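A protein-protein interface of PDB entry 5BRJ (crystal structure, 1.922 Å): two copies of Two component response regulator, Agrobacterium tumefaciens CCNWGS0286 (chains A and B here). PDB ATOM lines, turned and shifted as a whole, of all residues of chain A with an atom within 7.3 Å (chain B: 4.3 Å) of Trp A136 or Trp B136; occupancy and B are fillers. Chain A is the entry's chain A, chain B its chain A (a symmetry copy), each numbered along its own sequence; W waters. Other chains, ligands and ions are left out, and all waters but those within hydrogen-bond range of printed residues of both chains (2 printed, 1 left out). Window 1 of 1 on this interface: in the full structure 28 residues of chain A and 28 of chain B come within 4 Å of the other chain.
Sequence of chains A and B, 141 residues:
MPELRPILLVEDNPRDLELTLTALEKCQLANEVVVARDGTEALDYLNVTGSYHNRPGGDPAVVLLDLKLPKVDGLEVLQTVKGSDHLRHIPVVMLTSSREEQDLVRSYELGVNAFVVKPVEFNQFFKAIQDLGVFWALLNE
The backbone carbonyl oxygen of Cys A27 is in hydrogen-bond range of the side-chain amide nitrogen of Gln B130 (2.9 Å). O of Cys A27 lies within hydrogen-bond range of NE1 of Trp B136 (2.8 Å). OE1 of Gln B130 lies close to OE1 of Gln A28, at 3.5 Å. The backbone NH of Trp B136 sits at hydrogen-bond distance from the backbone carbonyl oxygen of Gln A28. The backbone carbonyl oxygen of Trp B136 is in hydrogen-bond range of the backbone NH of Ala A30. The backbone NH (N) of Leu B138 sits at hydrogen-bond distance from the side-chain amide oxygen (OD1) of Asn A31 (2.9 Å). The side-chain amide nitrogen (NE2) of Gln A130 lies within hydrogen-bond range of the backbone carbonyl oxygen (O) of Cys B27, 2.9 Å away. The side-chain amide oxygen of Gln A130 sits close to the side-chain amide oxygen of Gln B28 (3.5 Å). The indole nitrogen (NE1) of Trp A136 is in hydrogen-bond range of the backbone carbonyl oxygen (O) of Cys B27, at 2.8 Å. N of Trp A136 sits at hydrogen-bond distance from O of Gln B28 (3.0 Å). O of Trp A136 lies within hydrogen-bond range of N of Ala B30 (2.7 Å). O of Ala A137 lies within hydrogen-bond range of N of Ala B137 (3.0 Å). N of Leu A139 sits at hydrogen-bond distance from O of Phe B135, 2.9 Å away.
O of Ala A23 sits close to SG of Cys A27. The backbone carbonyl oxygen of Leu A24 is in hydrogen-bond range of the backbone NH of Leu A29, 3.4 Å away. O of Ile A129 sits at hydrogen-bond distance from N of Val A134 (3.3 Å).
Among the printed residues, merely in contact across the chains: Ala A137 with Trp B136, Trp A136 with Ala B137, Gln A28 with Phe B135, Phe A135 with Gln B28, Asn A31 with Ala B137, Leu A29 with Trp B136, Trp A136 with Leu B29, Gln A28 with Val B134, Val A134 with Gln B28, Phe A126 with Phe B126, Trp A136 with Phe B125, Phe A125 with Trp B136, Phe A122 with Phe B126, Ile A129 with Leu B138, Leu A138 with Phe B135, Phe A135 with Leu B138, Phe A122 with Gln B130, Leu A4 with Ala B137, Leu A138 with Val B134, Val A134 with Leu B138, Leu A139 with Val B134, Trp A136 with Trp B136, Gly A133 with Gln B28 and Lys A26 with Gln B130.
Of the printed residues of chain B, Gln A28 touches Gln B130 (3.5 Å), Val B134 (3.6 Å), Phe B135 (3.4 Å) and Trp B136 (3.0 Å). Of the printed residues of chain B, Ala A30 touches Trp B136. Trp A136 touches seven residues of chain B. Trp B136 touches just these residues of chain A: Cys A27 (2.8 Å), Gln A28 (3.0 Å), Leu A29 (3.4 Å), Ala A30 (2.7 Å), Phe A125 (3.6 Å), Trp A136 (3.9 Å) and Ala A137 (3.2 Å). The nearest residue of chain B that does not touch Trp A136 is Phe B126 (4.2 Å).
Printed residues of chain B that touch a printed residue of chain A: Cys B27, Gln B28, Leu B29, Ala B30, Phe B125, Phe B126, Gln B130, Val B134, Phe B135, Trp B136, Ala B137 and Leu B138. Hydrophobic or aromatic side chains of chain B within 4 Å of the printed part of chain A: Leu B29, Ala B30, Phe B125, Phe B126, Val B134, Phe B135, Trp B136, Ala B137 and Leu B138. Among the printed residues, no Asp or Glu carboxylate lies within 4 Å of a Lys or Arg side-chain nitrogen of the other chain.
Cys A27 touches Trp B136, and with the chains exchanged Trp A136 touches Cys B27. Phe B126 touches its own counterpart, Phe A126. Val A134 touches Leu B138, and with the chains exchanged Leu A138 touches Val B134.
Water W2 bridges the backbone carbonyl oxygen (O) of Val B134 (2.6 Å) and the side-chain amide oxygen (OE1) of Gln A28 (2.8 Å). Water W1 bridges the backbone carbonyl oxygen (O) of Leu A139 (2.9 Å) and the backbone NH (N) of Phe B135 (2.9 Å).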
ATOM      1  N   LEU A   4      22.762 -15.009  -2.967  1.00  0.00           N
ATOM      2  CA  LEU A   4      22.786 -13.861  -2.077  1.00  0.00           C
ATOM      3  C   LEU A   4      22.304 -12.637  -2.832  1.00  0.00           C
ATOM      4  O   LEU A   4      22.669 -12.449  -3.988  1.00  0.00           O
ATOM      5  CB  LEU A   4      24.186 -13.616  -1.542  1.00  0.00           C
ATOM      6  CG  LEU A   4      24.762 -14.677  -0.615  1.00  0.00           C
ATOM      7  CD1 LEU A   4      26.076 -14.167  -0.034  1.00  0.00           C
ATOM      8  CD2 LEU A   4      23.759 -15.008   0.476  1.00  0.00           C
ATOM      9  N   ALA A  23      34.546  -0.978   5.746  1.00  0.00           N
ATOM     10  CA  ALA A  23      34.039  -1.622   6.957  1.00  0.00           C
ATOM     11  C   ALA A  23      33.279  -2.889   6.619  1.00  0.00           C
ATOM     12  O   ALA A  23      33.407  -3.918   7.307  1.00  0.00           O
ATOM     13  CB  ALA A  23      33.143  -0.671   7.734  1.00  0.00           C
ATOM     14  N   LEU A  24      32.474  -2.817   5.566  1.00  0.00           N
ATOM     15  CA  LEU A  24      31.691  -3.978   5.149  1.00  0.00           C
ATOM     16  C   LEU A  24      32.608  -5.091   4.652  1.00  0.00           C
ATOM     17  O   LEU A  24      32.411  -6.266   4.974  1.00  0.00           O
ATOM     18  CB  LEU A  24      30.681  -3.588   4.068  1.00  0.00           C
ATOM     19  CG  LEU A  24      29.553  -2.671   4.559  1.00  0.00           C
ATOM     20  CD1 LEU A  24      28.637  -2.304   3.408  1.00  0.00           C
ATOM     21  CD2 LEU A  24      28.763  -3.337   5.686  1.00  0.00           C
ATOM     22  N   GLU A  25      33.626  -4.724   3.888  1.00  0.00           N
ATOM     23  CA  GLU A  25      34.583  -5.724   3.424  1.00  0.00           C
ATOM     24  C   GLU A  25      35.326  -6.359   4.590  1.00  0.00           C
ATOM     25  O   GLU A  25      35.482  -7.580   4.656  1.00  0.00           O
ATOM     26  CB  GLU A  25      35.591  -5.107   2.454  1.00  0.00           C
ATOM     27  CG  GLU A  25      36.547  -6.131   1.899  1.00  0.00           C
ATOM     28  CD  GLU A  25      37.414  -5.579   0.795  1.00  0.00           C
ATOM     29  OE1 GLU A  25      37.641  -4.348   0.773  1.00  0.00           O
ATOM     30  OE2 GLU A  25      37.861  -6.380  -0.054  1.00  0.00           O
ATOM     31  N   LYS A  26      35.775  -5.520   5.517  1.00  0.00           N
ATOM     32  CA  LYS A  26      36.594  -5.983   6.629  1.00  0.00           C
ATOM     33  C   LYS A  26      35.832  -6.764   7.691  1.00  0.00           C
ATOM     34  O   LYS A  26      36.450  -7.334   8.582  1.00  0.00           O
ATOM     35  CB  LYS A  26      37.301  -4.797   7.284  1.00  0.00           C
ATOM     36  CG  LYS A  26      38.435  -4.253   6.413  1.00  0.00           C
ATOM     37  CD  LYS A  26      39.618  -3.729   7.233  1.00  0.00           C
ATOM     38  CE  LYS A  26      39.379  -2.323   7.768  1.00  0.00           C
ATOM     39  NZ  LYS A  26      40.666  -1.586   7.984  1.00  0.00           N
ATOM     40  N   CYS A  27      34.504  -6.797   7.626  1.00  0.00           N
ATOM     41  CA  CYS A  27      33.772  -7.643   8.570  1.00  0.00           C
ATOM     42  C   CYS A  27      33.310  -8.914   7.874  1.00  0.00           C
ATOM     43  O   CYS A  27      32.498  -9.665   8.417  1.00  0.00           O
ATOM     44  CB  CYS A  27      32.589  -6.904   9.205  1.00  0.00           C
ATOM     45  SG  CYS A  27      31.145  -6.703   8.163  1.00  0.00           S
ATOM     46  N   GLN A  28      33.847  -9.146   6.677  1.00  0.00           N
ATOM     47  CA  GLN A  28      33.624 -10.383   5.921  1.00  0.00           C
ATOM     48  C   GLN A  28      32.156 -10.622   5.597  1.00  0.00           C
ATOM     49  O   GLN A  28      31.694 -11.764   5.600  1.00  0.00           O
ATOM     50  CB  GLN A  28      34.174 -11.604   6.681  1.00  0.00           C
ATOM     51  CG  GLN A  28      35.699 -11.693   6.753  1.00  0.00           C
ATOM     52  CD  GLN A  28      36.299 -10.661   7.686  1.00  0.00           C
ATOM     53  OE1 GLN A  28      35.935 -10.576   8.869  1.00  0.00           O
ATOM     54  NE2 GLN A  28      37.217  -9.863   7.162  1.00  0.00           N
ATOM     55  N   LEU A  29      31.422  -9.548   5.336  1.00  0.00           N
ATOM     56  CA  LEU A  29      30.073  -9.661   4.797  1.00  0.00           C
ATOM     57  C   LEU A  29      30.148 -10.101   3.338  1.00  0.00           C
ATOM     58  O   LEU A  29      30.792  -9.449   2.503  1.00  0.00           O
ATOM     59  CB  LEU A  29      29.324  -8.329   4.915  1.00  0.00           C
ATOM     60  CG  LEU A  29      27.899  -8.333   4.360  1.00  0.00           C
ATOM     61  CD1 LEU A  29      27.017  -9.284   5.168  1.00  0.00           C
ATOM     62  CD2 LEU A  29      27.341  -6.912   4.383  1.00  0.00           C
ATOM     63  N   ALA A  30      29.488 -11.204   3.022  1.00  0.00           N
ATOM     64  CA  ALA A  30      29.637 -11.808   1.703  1.00  0.00           C
ATOM     65  C   ALA A  30      28.807 -11.137   0.602  1.00  0.00           C
ATOM     66  O   ALA A  30      29.225 -11.138  -0.551  1.00  0.00           O
ATOM     67  CB  ALA A  30      29.291 -13.280   1.779  1.00  0.00           C
ATOM     68  N   ASN A  31      27.632 -10.603   0.943  1.00  0.00           N
ATOM     69  CA  ASN A  31      26.777  -9.939  -0.046  1.00  0.00           C
ATOM     70  C   ASN A  31      27.521  -8.846  -0.798  1.00  0.00           C
ATOM     71  O   ASN A  31      28.206  -8.038  -0.186  1.00  0.00           O
ATOM     72  CB  ASN A  31      25.553  -9.306   0.614  1.00  0.00           C
ATOM     73  CG  ASN A  31      24.819 -10.263   1.510  1.00  0.00           C
ATOM     74  OD1 ASN A  31      25.356 -10.712   2.519  1.00  0.00           O
ATOM     75  ND2 ASN A  31      23.576 -10.573   1.158  1.00  0.00           N
ATOM     76  N   PHE A 122      31.338  -2.604  12.613  1.00  0.00           N
ATOM     77  CA  PHE A 122      30.506  -3.812  12.545  1.00  0.00           C
ATOM     78  C   PHE A 122      29.565  -3.998  13.734  1.00  0.00           C
ATOM     79  O   PHE A 122      28.478  -4.550  13.564  1.00  0.00           O
ATOM     80  CB  PHE A 122      31.364  -5.084  12.336  1.00  0.00           C
ATOM     81  CG  PHE A 122      32.168  -5.515  13.541  1.00  0.00           C
ATOM     82  CD1 PHE A 122      31.566  -6.137  14.624  1.00  0.00           C
ATOM     83  CD2 PHE A 122      33.546  -5.368  13.544  1.00  0.00           C
ATOM     84  CE1 PHE A 122      32.314  -6.544  15.722  1.00  0.00           C
ATOM     85  CE2 PHE A 122      34.301  -5.778  14.634  1.00  0.00           C
ATOM     86  CZ  PHE A 122      33.684  -6.362  15.722  1.00  0.00           C
ATOM     87  N   PHE A 125      26.611  -1.958  13.083  1.00  0.00           N
ATOM     88  CA  PHE A 125      25.984  -2.495  11.875  1.00  0.00           C
ATOM     89  C   PHE A 125      25.192  -3.749  12.198  1.00  0.00           C
ATOM     90  O   PHE A 125      24.035  -3.881  11.813  1.00  0.00           O
ATOM     91  CB  PHE A 125      27.024  -2.800  10.783  1.00  0.00           C
ATOM     92  CG  PHE A 125      26.423  -3.367   9.522  1.00  0.00           C
ATOM     93  CD1 PHE A 125      25.488  -2.644   8.800  1.00  0.00           C
ATOM     94  CD2 PHE A 125      26.784  -4.622   9.061  1.00  0.00           C
ATOM     95  CE1 PHE A 125      24.924  -3.166   7.643  1.00  0.00           C
ATOM     96  CE2 PHE A 125      26.222  -5.144   7.903  1.00  0.00           C
ATOM     97  CZ  PHE A 125      25.293  -4.419   7.202  1.00  0.00           C
ATOM     98  N   PHE A 126      25.808  -4.674  12.923  1.00  0.00           N
ATOM     99  CA  PHE A 126      25.117  -5.919  13.241  1.00  0.00           C
ATOM    100  C   PHE A 126      23.909  -5.668  14.137  1.00  0.00           C
ATOM    101  O   PHE A 126      22.871  -6.297  13.980  1.00  0.00           O
ATOM    102  CB  PHE A 126      26.070  -6.920  13.900  1.00  0.00           C
ATOM    103  CG  PHE A 126      25.476  -8.287  14.050  1.00  0.00           C
ATOM    104  CD1 PHE A 126      25.208  -9.060  12.928  1.00  0.00           C
ATOM    105  CD2 PHE A 126      25.170  -8.791  15.301  1.00  0.00           C
ATOM    106  CE1 PHE A 126      24.653 -10.327  13.048  1.00  0.00           C
ATOM    107  CE2 PHE A 126      24.611 -10.070  15.440  1.00  0.00           C
ATOM    108  CZ  PHE A 126      24.353 -10.833  14.313  1.00  0.00           C
ATOM    109  N   ILE A 129      21.136  -4.736  11.937  1.00  0.00           N
ATOM    110  CA  ILE A 129      20.642  -5.979  11.358  1.00  0.00           C
ATOM    111  C   ILE A 129      19.684  -6.671  12.326  1.00  0.00           C
ATOM    112  O   ILE A 129      18.611  -7.148  11.929  1.00  0.00           O
ATOM    113  CB  ILE A 129      21.808  -6.931  11.002  1.00  0.00           C
ATOM    114  CG1 ILE A 129      22.660  -6.334   9.884  1.00  0.00           C
ATOM    115  CG2 ILE A 129      21.298  -8.332  10.656  1.00  0.00           C
ATOM    116  CD1 ILE A 129      21.855  -5.775   8.728  1.00  0.00           C
ATOM    117  N   GLN A 130      20.074  -6.715  13.596  1.00  0.00           N
ATOM    118  CA  GLN A 130      19.259  -7.332  14.634  1.00  0.00           C
ATOM    119  C   GLN A 130      17.969  -6.539  14.833  1.00  0.00           C
ATOM    120  O   GLN A 130      16.878  -7.115  14.939  1.00  0.00           O
ATOM    121  CB  GLN A 130      20.052  -7.428  15.942  1.00  0.00           C
ATOM    122  CG  GLN A 130      21.139  -8.514  15.899  1.00  0.00           C
ATOM    123  CD  GLN A 130      20.541  -9.868  15.597  1.00  0.00           C
ATOM    124  OE1 GLN A 130      19.544 -10.248  16.191  1.00  0.00           O
ATOM    125  NE2 GLN A 130      21.125 -10.589  14.652  1.00  0.00           N
ATOM    126  N   GLY A 133      15.418  -7.499  12.264  1.00  0.00           N
ATOM    127  CA  GLY A 133      14.925  -8.861  12.206  1.00  0.00           C
ATOM    128  C   GLY A 133      15.361  -9.594  10.951  1.00  0.00           C
ATOM    129  O   GLY A 133      14.710 -10.544  10.528  1.00  0.00           O
ATOM    130  N   VAL A 134      16.468  -9.164  10.352  1.00  0.00           N
ATOM    131  CA  VAL A 134      16.955  -9.789   9.125  1.00  0.00           C
ATOM    132  C   VAL A 134      17.680 -11.090   9.460  1.00  0.00           C
ATOM    133  O   VAL A 134      18.428 -11.137  10.430  1.00  0.00           O
ATOM    134  CB  VAL A 134      17.894  -8.839   8.353  1.00  0.00           C
ATOM    135  CG1 VAL A 134      18.600  -9.555   7.206  1.00  0.00           C
ATOM    136  CG2 VAL A 134      17.099  -7.639   7.820  1.00  0.00           C
ATOM    137  N   PHE A 135      17.442 -12.142   8.678  1.00  0.00           N
ATOM    138  CA  PHE A 135      18.139 -13.404   8.895  1.00  0.00           C
ATOM    139  C   PHE A 135      19.563 -13.344   8.355  1.00  0.00           C
ATOM    140  O   PHE A 135      19.844 -12.671   7.361  1.00  0.00           O
ATOM    141  CB  PHE A 135      17.378 -14.565   8.252  1.00  0.00           C
ATOM    142  CG  PHE A 135      16.182 -15.012   9.049  1.00  0.00           C
ATOM    143  CD1 PHE A 135      14.979 -14.336   8.957  1.00  0.00           C
ATOM    144  CD2 PHE A 135      16.268 -16.099   9.901  1.00  0.00           C
ATOM    145  CE1 PHE A 135      13.884 -14.742   9.695  1.00  0.00           C
ATOM    146  CE2 PHE A 135      15.176 -16.507  10.634  1.00  0.00           C
ATOM    147  CZ  PHE A 135      13.986 -15.834  10.529  1.00  0.00           C
ATOM    148  N   TRP A 136      20.465 -14.059   9.014  1.00  0.00           N
ATOM    149  CA  TRP A 136      21.859 -14.033   8.618  1.00  0.00           C
ATOM    150  C   TRP A 136      22.444 -15.425   8.770  1.00  0.00           C
ATOM    151  O   TRP A 136      21.872 -16.286   9.443  1.00  0.00           O
ATOM    152  CB  TRP A 136      22.646 -12.998   9.432  1.00  0.00           C
ATOM    153  CG  TRP A 136      22.793 -13.339  10.884  1.00  0.00           C
ATOM    154  CD1 TRP A 136      21.816 -13.320  11.834  1.00  0.00           C
ATOM    155  CD2 TRP A 136      23.995 -13.746  11.547  1.00  0.00           C
ATOM    156  NE1 TRP A 136      22.334 -13.711  13.053  1.00  0.00           N
ATOM    157  CE2 TRP A 136      23.672 -13.965  12.904  1.00  0.00           C
ATOM    158  CE3 TRP A 136      25.312 -13.946  11.125  1.00  0.00           C
ATOM    159  CZ2 TRP A 136      24.620 -14.374  13.842  1.00  0.00           C
ATOM    160  CZ3 TRP A 136      26.253 -14.343  12.055  1.00  0.00           C
ATOM    161  CH2 TRP A 136      25.901 -14.555  13.400  1.00  0.00           C
ATOM    162  N   ALA A 137      23.573 -15.651   8.121  1.00  0.00           N
ATOM    163  CA  ALA A 137      24.123 -16.988   8.061  1.00  0.00           C
ATOM    164  C   ALA A 137      25.627 -16.952   8.134  1.00  0.00           C
ATOM    165  O   ALA A 137      26.252 -16.001   7.681  1.00  0.00           O
ATOM    166  CB  ALA A 137      23.682 -17.680   6.784  1.00  0.00           C
ATOM    167  N   LEU A 138      26.203 -18.004   8.701  1.00  0.00           N
ATOM    168  CA  LEU A 138      27.641 -18.213   8.626  1.00  0.00           C
ATOM    169  C   LEU A 138      27.959 -19.077   7.405  1.00  0.00           C
ATOM    170  O   LEU A 138      27.298 -20.089   7.164  1.00  0.00           O
ATOM    171  CB  LEU A 138      28.149 -18.881   9.909  1.00  0.00           C
ATOM    172  CG  LEU A 138      27.969 -18.051  11.178  1.00  0.00           C
ATOM    173  CD1 LEU A 138      28.252 -18.880  12.426  1.00  0.00           C
ATOM    174  CD2 LEU A 138      28.863 -16.805  11.139  1.00  0.00           C
ATOM    175  N   LEU A 139      28.962 -18.673   6.633  1.00  0.00           N
ATOM    176  CA  LEU A 139      29.354 -19.417   5.436  1.00  0.00           C
ATOM    177  C   LEU A 139      30.633 -20.222   5.681  1.00  0.00           C
ATOM    178  O   LEU A 139      31.396 -19.929   6.606  1.00  0.00           O
ATOM    179  CB  LEU A 139      29.552 -18.466   4.257  1.00  0.00           C
ATOM    180  CG  LEU A 139      28.383 -17.518   3.984  1.00  0.00           C
ATOM    181  CD1 LEU A 139      28.690 -16.635   2.781  1.00  0.00           C
ATOM    182  CD2 LEU A 139      27.110 -18.324   3.758  1.00  0.00           C
ATOM    183  N   GLU A 141      32.370 -21.205   2.703  1.00  0.00           N
ATOM    184  CA  GLU A 141      33.049 -20.710   1.498  1.00  0.00           C
ATOM    185  C   GLU A 141      34.082 -21.678   0.921  1.00  0.00           C
ATOM    186  O   GLU A 141      34.267 -21.746  -0.298  1.00  0.00           O
ATOM    187  CB  GLU A 141      33.710 -19.355   1.778  1.00  0.00           C
ATOM    188  CG  GLU A 141      32.762 -18.181   1.607  1.00  0.00           C
ATOM    189  CD  GLU A 141      33.396 -17.017   0.853  1.00  0.00           C
ATOM    190  OE1 GLU A 141      34.626 -17.034   0.640  1.00  0.00           O
ATOM    191  OE2 GLU A 141      32.661 -16.082   0.472  1.00  0.00           O
ATOM    192  N   CYS B  27      18.533 -14.330  17.405  1.00  0.00           N
ATOM    193  CA  CYS B  27      19.305 -13.370  16.614  1.00  0.00           C
ATOM    194  C   CYS B  27      19.197 -13.712  15.136  1.00  0.00           C
ATOM    195  O   CYS B  27      19.935 -13.169  14.313  1.00  0.00           O
ATOM    196  CB  CYS B  27      20.771 -13.308  17.058  1.00  0.00           C
ATOM    197  SG  CYS B  27      21.803 -14.676  16.529  1.00  0.00           S
ATOM    198  N   GLN B  28      18.262 -14.605  14.816  1.00  0.00           N
ATOM    199  CA  GLN B  28      17.923 -14.956  13.433  1.00  0.00           C
ATOM    200  C   GLN B  28      19.105 -15.529  12.662  1.00  0.00           C
ATOM    201  O   GLN B  28      19.253 -15.271  11.467  1.00  0.00           O
ATOM    202  CB  GLN B  28      17.373 -13.737  12.671  1.00  0.00           C
ATOM    203  CG  GLN B  28      15.980 -13.275  13.101  1.00  0.00           C
ATOM    204  CD  GLN B  28      15.981 -12.606  14.460  1.00  0.00           C
ATOM    205  OE1 GLN B  28      16.717 -11.637  14.698  1.00  0.00           O
ATOM    206  NE2 GLN B  28      15.163 -13.121  15.365  1.00  0.00           N
ATOM    207  N   LEU B  29      19.950 -16.288  13.347  1.00  0.00           N
ATOM    208  CA  LEU B  29      20.982 -17.071  12.680  1.00  0.00           C
ATOM    209  C   LEU B  29      20.335 -18.249  11.958  1.00  0.00           C
ATOM    210  O   LEU B  29      19.632 -19.067  12.568  1.00  0.00           O
ATOM    211  CB  LEU B  29      22.025 -17.569  13.685  1.00  0.00           C
ATOM    212  CG  LEU B  29      23.149 -18.418  13.089  1.00  0.00           C
ATOM    213  CD1 LEU B  29      23.989 -17.585  12.122  1.00  0.00           C
ATOM    214  CD2 LEU B  29      24.008 -18.987  14.216  1.00  0.00           C
ATOM    215  N   ALA B  30      20.571 -18.344  10.659  1.00  0.00           N
ATOM    216  CA  ALA B  30      19.862 -19.323   9.843  1.00  0.00           C
ATOM    217  C   ALA B  30      20.426 -20.747   9.931  1.00  0.00           C
ATOM    218  O   ALA B  30      19.670 -21.703   9.794  1.00  0.00           O
ATOM    219  CB  ALA B  30      19.849 -18.866   8.400  1.00  0.00           C
ATOM    220  N   PHE B 125      28.687 -12.776  20.564  1.00  0.00           N
ATOM    221  CA  PHE B 125      28.740 -13.862  19.585  1.00  0.00           C
ATOM    222  C   PHE B 125      29.268 -13.354  18.255  1.00  0.00           C
ATOM    223  O   PHE B 125      30.170 -13.943  17.669  1.00  0.00           O
ATOM    224  CB  PHE B 125      27.361 -14.514  19.386  1.00  0.00           C
ATOM    225  CG  PHE B 125      27.366 -15.633  18.376  1.00  0.00           C
ATOM    226  CD1 PHE B 125      28.162 -16.751  18.565  1.00  0.00           C
ATOM    227  CD2 PHE B 125      26.585 -15.567  17.234  1.00  0.00           C
ATOM    228  CE1 PHE B 125      28.177 -17.780  17.632  1.00  0.00           C
ATOM    229  CE2 PHE B 125      26.599 -16.596  16.301  1.00  0.00           C
ATOM    230  CZ  PHE B 125      27.395 -17.694  16.500  1.00  0.00           C
ATOM    231  N   PHE B 126      28.717 -12.246  17.777  1.00  0.00           N
ATOM    232  CA  PHE B 126      29.152 -11.722  16.488  1.00  0.00           C
ATOM    233  C   PHE B 126      30.608 -11.271  16.538  1.00  0.00           C
ATOM    234  O   PHE B 126      31.356 -11.464  15.587  1.00  0.00           O
ATOM    235  CB  PHE B 126      28.254 -10.569  16.034  1.00  0.00           C
ATOM    236  CG  PHE B 126      28.517 -10.137  14.625  1.00  0.00           C
ATOM    237  CD1 PHE B 126      28.212 -10.982  13.565  1.00  0.00           C
ATOM    238  CD2 PHE B 126      29.081  -8.902  14.357  1.00  0.00           C
ATOM    239  CE1 PHE B 126      28.455 -10.600  12.252  1.00  0.00           C
ATOM    240  CE2 PHE B 126      29.330  -8.500  13.037  1.00  0.00           C
ATOM    241  CZ  PHE B 126      29.018  -9.351  11.990  1.00  0.00           C
ATOM    242  N   GLN B 130      33.691 -12.354  14.207  1.00  0.00           N
ATOM    243  CA  GLN B 130      34.624 -11.402  13.622  1.00  0.00           C
ATOM    244  C   GLN B 130      36.060 -11.783  13.978  1.00  0.00           C
ATOM    245  O   GLN B 130      36.953 -11.764  13.121  1.00  0.00           O
ATOM    246  CB  GLN B 130      34.299  -9.982  14.098  1.00  0.00           C
ATOM    247  CG  GLN B 130      33.030  -9.412  13.445  1.00  0.00           C
ATOM    248  CD  GLN B 130      33.153  -9.399  11.940  1.00  0.00           C
ATOM    249  OE1 GLN B 130      34.167  -8.973  11.408  1.00  0.00           O
ATOM    250  NE2 GLN B 130      32.139  -9.893  11.246  1.00  0.00           N
ATOM    251  N   VAL B 134      35.350 -15.411  10.032  1.00  0.00           N
ATOM    252  CA  VAL B 134      34.356 -16.217   9.329  1.00  0.00           C
ATOM    253  C   VAL B 134      33.489 -15.320   8.450  1.00  0.00           C
ATOM    254  O   VAL B 134      33.107 -14.236   8.878  1.00  0.00           O
ATOM    255  CB  VAL B 134      33.476 -17.003  10.322  1.00  0.00           C
ATOM    256  CG1 VAL B 134      32.285 -17.655   9.626  1.00  0.00           C
ATOM    257  CG2 VAL B 134      34.319 -18.067  11.039  1.00  0.00           C
ATOM    258  N   PHE B 135      33.200 -15.757   7.225  1.00  0.00           N
ATOM    259  CA  PHE B 135      32.329 -14.986   6.346  1.00  0.00           C
ATOM    260  C   PHE B 135      30.865 -15.158   6.736  1.00  0.00           C
ATOM    261  O   PHE B 135      30.448 -16.217   7.209  1.00  0.00           O
ATOM    262  CB  PHE B 135      32.539 -15.386   4.884  1.00  0.00           C
ATOM    263  CG  PHE B 135      33.783 -14.800   4.274  1.00  0.00           C
ATOM    264  CD1 PHE B 135      35.017 -15.391   4.482  1.00  0.00           C
ATOM    265  CD2 PHE B 135      33.719 -13.651   3.506  1.00  0.00           C
ATOM    266  CE1 PHE B 135      36.160 -14.848   3.929  1.00  0.00           C
ATOM    267  CE2 PHE B 135      34.858 -13.112   2.951  1.00  0.00           C
ATOM    268  CZ  PHE B 135      36.074 -13.710   3.158  1.00  0.00           C
ATOM    269  N   TRP B 136      30.082 -14.109   6.528  1.00  0.00           N
ATOM    270  CA  TRP B 136      28.684 -14.145   6.910  1.00  0.00           C
ATOM    271  C   TRP B 136      27.864 -13.419   5.860  1.00  0.00           C
ATOM    272  O   TRP B 136      28.398 -12.664   5.044  1.00  0.00           O
ATOM    273  CB  TRP B 136      28.478 -13.541   8.305  1.00  0.00           C
ATOM    274  CG  TRP B 136      28.731 -12.066   8.381  1.00  0.00           C
ATOM    275  CD1 TRP B 136      29.937 -11.436   8.305  1.00  0.00           C
ATOM    276  CD2 TRP B 136      27.748 -11.039   8.554  1.00  0.00           C
ATOM    277  NE1 TRP B 136      29.765 -10.069   8.401  1.00  0.00           N
ATOM    278  CE2 TRP B 136      28.431  -9.803   8.567  1.00  0.00           C
ATOM    279  CE3 TRP B 136      26.358 -11.045   8.698  1.00  0.00           C
ATOM    280  CZ2 TRP B 136      27.770  -8.585   8.720  1.00  0.00           C
ATOM    281  CZ3 TRP B 136      25.704  -9.839   8.857  1.00  0.00           C
ATOM    282  CH2 TRP B 136      26.410  -8.624   8.865  1.00  0.00           C
ATOM    283  N   ALA B 137      26.566 -13.670   5.866  1.00  0.00           N
ATOM    284  CA  ALA B 137      25.723 -13.164   4.805  1.00  0.00           C
ATOM    285  C   ALA B 137      24.379 -12.748   5.342  1.00  0.00           C
ATOM    286  O   ALA B 137      23.888 -13.317   6.309  1.00  0.00           O
ATOM    287  CB  ALA B 137      25.545 -14.219   3.728  1.00  0.00           C
ATOM    288  N   LEU B 138      23.783 -11.753   4.698  1.00  0.00           N
ATOM    289  CA  LEU B 138      22.392 -11.409   4.954  1.00  0.00           C
ATOM    290  C   LEU B 138      21.497 -12.175   3.979  1.00  0.00           C
ATOM    291  O   LEU B 138      21.781 -12.231   2.781  1.00  0.00           O
ATOM    292  CB  LEU B 138      22.182  -9.897   4.809  1.00  0.00           C
ATOM    293  CG  LEU B 138      22.958  -9.043   5.809  1.00  0.00           C
ATOM    294  CD1 LEU B 138      22.904  -7.566   5.435  1.00  0.00           C
ATOM    295  CD2 LEU B 138      22.427  -9.263   7.232  1.00  0.00           C
HETATM  296  O   HOH W   1      33.918 -18.476   6.341  1.00  0.00           O
HETATM  297  O   HOH W   2      34.379 -12.487  10.242  1.00  0.00           O
